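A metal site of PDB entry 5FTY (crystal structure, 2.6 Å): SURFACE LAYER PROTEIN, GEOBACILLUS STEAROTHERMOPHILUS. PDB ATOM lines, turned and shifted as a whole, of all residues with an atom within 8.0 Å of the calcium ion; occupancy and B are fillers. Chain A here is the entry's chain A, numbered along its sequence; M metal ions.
Within 4 Å of the calcium ion: Asp 18, Asp 19, Lys 21, Asn 32 and Asp 34. The nearest printed residue that does not touch the calcium ion is Val 35 (4.5 Å).
The calcium ion is bound by OD1 of Asn 32 (2.3 Å), O of Asp 34 (2.4 Å), OD2 of Asp 18 (2.4 Å), OD1 of Asp 19 (2.4 Å) and O of Lys 21 (2.7 Å).
The backbone carbonyl oxygen (O) of Asn 32 is in hydrogen-bond range of the backbone NH (N) of Asp 23, 2.6 Å away. OD1 of Asp 34 lies within hydrogen-bond range of NE2 of Gln 36 (2.9 Å). The side-chain carboxylate (OD2) of Asp 18 sits close to the backbone NH (N) of Gly 20 (3.3 Å). The backbone NH of Gln 36 lies within hydrogen-bond range of the side-chain carboxylate of Asp 18 (2.7 Å). The side-chain carboxylate (OE1) of Glu 113 lies within salt-bridge range of the side-chain amino group (NZ) of Lys 21 (2.9 Å).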
ATOM      1  N   VAL A  16      22.709  19.710  13.092  1.00  0.00           N
ATOM      2  CA  VAL A  16      21.655  20.127  12.182  1.00  0.00           C
ATOM      3  C   VAL A  16      21.007  21.396  12.708  1.00  0.00           C
ATOM      4  O   VAL A  16      20.377  21.396  13.766  1.00  0.00           O
ATOM      5  CB  VAL A  16      20.573  19.028  12.030  1.00  0.00           C
ATOM      6  CG1 VAL A  16      19.428  19.529  11.164  1.00  0.00           C
ATOM      7  CG2 VAL A  16      21.170  17.749  11.461  1.00  0.00           C
ATOM      8  N   LEU A  17      21.179  22.489  11.980  1.00  0.00           N
ATOM      9  CA  LEU A  17      20.666  23.781  12.426  1.00  0.00           C
ATOM     10  C   LEU A  17      19.151  23.900  12.247  1.00  0.00           C
ATOM     11  O   LEU A  17      18.492  24.593  13.008  1.00  0.00           O
ATOM     12  CB  LEU A  17      21.384  24.932  11.700  1.00  0.00           C
ATOM     13  CG  LEU A  17      22.895  25.069  11.912  1.00  0.00           C
ATOM     14  CD1 LEU A  17      23.417  26.298  11.200  1.00  0.00           C
ATOM     15  CD2 LEU A  17      23.246  25.111  13.397  1.00  0.00           C
ATOM     16  N   ASP A  18      18.613  23.219  11.242  1.00  0.00           N
ATOM     17  CA  ASP A  18      17.186  23.314  10.934  1.00  0.00           C
ATOM     18  C   ASP A  18      16.403  22.086  11.342  1.00  0.00           C
ATOM     19  O   ASP A  18      16.697  21.457  12.366  1.00  0.00           O
ATOM     20  CB  ASP A  18      16.979  23.597   9.442  1.00  0.00           C
ATOM     21  CG  ASP A  18      17.657  22.568   8.562  1.00  0.00           C
ATOM     22  OD1 ASP A  18      18.816  22.193   8.846  1.00  0.00           O
ATOM     23  OD2 ASP A  18      17.012  22.141   7.573  1.00  0.00           O
ATOM     24  N   ASP A  19      15.403  21.729  10.541  1.00  0.00           N
ATOM     25  CA  ASP A  19      14.544  20.576  10.818  1.00  0.00           C
ATOM     26  C   ASP A  19      15.098  19.324  10.147  1.00  0.00           C
ATOM     27  O   ASP A  19      14.520  18.238  10.267  1.00  0.00           O
ATOM     28  CB  ASP A  19      13.117  20.848  10.349  1.00  0.00           C
ATOM     29  CG  ASP A  19      13.026  21.027   8.843  1.00  0.00           C
ATOM     30  OD1 ASP A  19      14.036  21.431   8.235  1.00  0.00           O
ATOM     31  OD2 ASP A  19      11.948  20.756   8.266  1.00  0.00           O
ATOM     32  N   GLY A  20      16.204  19.477   9.428  1.00  0.00           N
ATOM     33  CA  GLY A  20      16.845  18.351   8.756  1.00  0.00           C
ATOM     34  C   GLY A  20      16.040  17.812   7.592  1.00  0.00           C
ATOM     35  O   GLY A  20      16.342  16.724   7.082  1.00  0.00           O
ATOM     36  N   LYS A  21      15.017  18.543   7.164  1.00  0.00           N
ATOM     37  CA  LYS A  21      14.183  18.099   6.056  1.00  0.00           C
ATOM     38  C   LYS A  21      14.221  19.073   4.888  1.00  0.00           C
ATOM     39  O   LYS A  21      14.393  20.280   5.075  1.00  0.00           O
ATOM     40  CB  LYS A  21      12.739  17.906   6.510  1.00  0.00           C
ATOM     41  CG  LYS A  21      12.556  16.979   7.700  1.00  0.00           C
ATOM     42  CD  LYS A  21      11.086  16.801   8.038  1.00  0.00           C
ATOM     43  CE  LYS A  21      10.884  16.140   9.391  1.00  0.00           C
ATOM     44  NZ  LYS A  21      11.546  14.800   9.461  1.00  0.00           N
ATOM     45  N   ILE A  22      14.071  18.539   3.681  1.00  0.00           N
ATOM     46  CA  ILE A  22      13.996  19.358   2.480  1.00  0.00           C
ATOM     47  C   ILE A  22      12.657  19.106   1.785  1.00  0.00           C
ATOM     48  O   ILE A  22      12.402  18.005   1.294  1.00  0.00           O
ATOM     49  CB  ILE A  22      15.133  19.030   1.497  1.00  0.00           C
ATOM     50  CG1 ILE A  22      16.479  19.387   2.111  1.00  0.00           C
ATOM     51  CG2 ILE A  22      14.927  19.771   0.183  1.00  0.00           C
ATOM     52  CD1 ILE A  22      17.656  18.870   1.317  1.00  0.00           C
ATOM     53  N   ASP A  23      11.799  20.130   1.748  1.00  0.00           N
ATOM     54  CA  ASP A  23      10.499  19.973   1.115  1.00  0.00           C
ATOM     55  C   ASP A  23      10.602  20.049  -0.407  1.00  0.00           C
ATOM     56  O   ASP A  23      11.052  21.048  -0.959  1.00  0.00           O
ATOM     57  CB  ASP A  23       9.507  21.031   1.633  1.00  0.00           C
ATOM     58  CG  ASP A  23       8.061  20.558   1.572  1.00  0.00           C
ATOM     59  OD1 ASP A  23       7.775  19.622   0.788  1.00  0.00           O
ATOM     60  OD2 ASP A  23       7.219  21.116   2.304  1.00  0.00           O
ATOM     61  N   ALA A  31       9.184  28.430   3.470  1.00  0.00           N
ATOM     62  CA  ALA A  31      10.023  27.695   2.537  1.00  0.00           C
ATOM     63  C   ALA A  31      11.001  26.783   3.263  1.00  0.00           C
ATOM     64  O   ALA A  31      11.778  27.231   4.101  1.00  0.00           O
ATOM     65  CB  ALA A  31      10.757  28.662   1.622  1.00  0.00           C
ATOM     66  N   ASN A  32      10.931  25.491   2.952  1.00  0.00           N
ATOM     67  CA  ASN A  32      11.763  24.494   3.605  1.00  0.00           C
ATOM     68  C   ASN A  32      12.654  23.797   2.577  1.00  0.00           C
ATOM     69  O   ASN A  32      12.541  22.594   2.361  1.00  0.00           O
ATOM     70  CB  ASN A  32      10.863  23.470   4.304  1.00  0.00           C
ATOM     71  CG  ASN A  32      11.620  22.626   5.311  1.00  0.00           C
ATOM     72  OD1 ASN A  32      12.838  22.699   5.398  1.00  0.00           O
ATOM     73  ND2 ASN A  32      10.893  21.830   6.086  1.00  0.00           N
ATOM     74  N   ASN A  33      13.556  24.559   1.971  1.00  0.00           N
ATOM     75  CA  ASN A  33      14.315  24.089   0.808  1.00  0.00           C
ATOM     76  C   ASN A  33      15.758  23.654   1.042  1.00  0.00           C
ATOM     77  O   ASN A  33      16.502  23.435   0.082  1.00  0.00           O
ATOM     78  CB  ASN A  33      14.273  25.145  -0.302  1.00  0.00           C
ATOM     79  CG  ASN A  33      12.908  25.279  -0.946  1.00  0.00           C
ATOM     80  OD1 ASN A  33      12.190  24.299  -1.087  1.00  0.00           O
ATOM     81  ND2 ASN A  33      12.567  26.485  -1.353  1.00  0.00           N
ATOM     82  N   ASP A  34      16.171  23.538   2.306  1.00  0.00           N
ATOM     83  CA  ASP A  34      17.538  23.107   2.591  1.00  0.00           C
ATOM     84  C   ASP A  34      17.723  22.478   3.971  1.00  0.00           C
ATOM     85  O   ASP A  34      16.842  22.540   4.821  1.00  0.00           O
ATOM     86  CB  ASP A  34      18.542  24.258   2.399  1.00  0.00           C
ATOM     87  CG  ASP A  34      18.293  25.419   3.359  1.00  0.00           C
ATOM     88  OD1 ASP A  34      18.144  25.193   4.576  1.00  0.00           O
ATOM     89  OD2 ASP A  34      18.264  26.577   2.881  1.00  0.00           O
ATOM     90  N   VAL A  35      18.889  21.855   4.169  1.00  0.00           N
ATOM     91  CA  VAL A  35      19.323  21.426   5.491  1.00  0.00           C
ATOM     92  C   VAL A  35      20.634  22.136   5.807  1.00  0.00           C
ATOM     93  O   VAL A  35      21.515  22.205   4.959  1.00  0.00           O
ATOM     94  CB  VAL A  35      19.563  19.900   5.556  1.00  0.00           C
ATOM     95  CG1 VAL A  35      20.057  19.499   6.945  1.00  0.00           C
ATOM     96  CG2 VAL A  35      18.304  19.139   5.179  1.00  0.00           C
ATOM     97  N   GLN A  36      20.755  22.655   7.022  1.00  0.00           N
ATOM     98  CA  GLN A  36      21.963  23.382   7.391  1.00  0.00           C
ATOM     99  C   GLN A  36      22.837  22.569   8.341  1.00  0.00           C
ATOM    100  O   GLN A  36      22.368  22.096   9.373  1.00  0.00           O
ATOM    101  CB  GLN A  36      21.607  24.736   7.995  1.00  0.00           C
ATOM    102  CG  GLN A  36      20.901  25.658   7.008  1.00  0.00           C
ATOM    103  CD  GLN A  36      19.850  26.531   7.667  1.00  0.00           C
ATOM    104  OE1 GLN A  36      20.089  27.131   8.711  1.00  0.00           O
ATOM    105  NE2 GLN A  36      18.680  26.608   7.055  1.00  0.00           N
ATOM    106  N   ILE A  85      22.578  21.786   2.293  1.00  0.00           N
ATOM    107  CA  ILE A  85      22.122  20.649   1.507  1.00  0.00           C
ATOM    108  C   ILE A  85      20.841  20.992   0.764  1.00  0.00           C
ATOM    109  O   ILE A  85      19.808  21.245   1.372  1.00  0.00           O
ATOM    110  CB  ILE A  85      21.868  19.413   2.392  1.00  0.00           C
ATOM    111  CG1 ILE A  85      22.983  19.245   3.431  1.00  0.00           C
ATOM    112  CG2 ILE A  85      21.715  18.167   1.535  1.00  0.00           C
ATOM    113  CD1 ILE A  85      24.360  19.071   2.830  1.00  0.00           C
ATOM    114  N   GLU A 113      16.438  14.338   5.216  1.00  0.00           N
ATOM    115  CA  GLU A 113      15.201  13.734   4.708  1.00  0.00           C
ATOM    116  C   GLU A 113      14.500  14.621   3.691  1.00  0.00           C
ATOM    117  O   GLU A 113      14.251  15.796   3.935  1.00  0.00           O
ATOM    118  CB  GLU A 113      14.260  13.390   5.870  1.00  0.00           C
ATOM    119  CG  GLU A 113      12.995  12.661   5.450  1.00  0.00           C
ATOM    120  CD  GLU A 113      12.109  12.292   6.625  1.00  0.00           C
ATOM    121  OE1 GLU A 113      12.467  12.639   7.775  1.00  0.00           O
ATOM    122  OE2 GLU A 113      11.061  11.655   6.407  1.00  0.00           O
ATOM    123  N   ILE A 115      11.066  15.433   1.853  1.00  0.00           N
ATOM    124  CA  ILE A 115       9.632  15.242   2.008  1.00  0.00           C
ATOM    125  C   ILE A 115       8.865  16.003   0.917  1.00  0.00           C
ATOM    126  O   ILE A 115       9.425  16.866   0.250  1.00  0.00           O
ATOM    127  CB  ILE A 115       9.134  15.736   3.381  1.00  0.00           C
ATOM    128  CG1 ILE A 115       9.366  17.237   3.534  1.00  0.00           C
ATOM    129  CG2 ILE A 115       9.822  14.973   4.497  1.00  0.00           C
ATOM    130  CD1 ILE A 115       8.836  17.800   4.831  1.00  0.00           C
HETATM  131 CA    CA M   1      14.989  22.580   6.309  1.00  0.00          CA
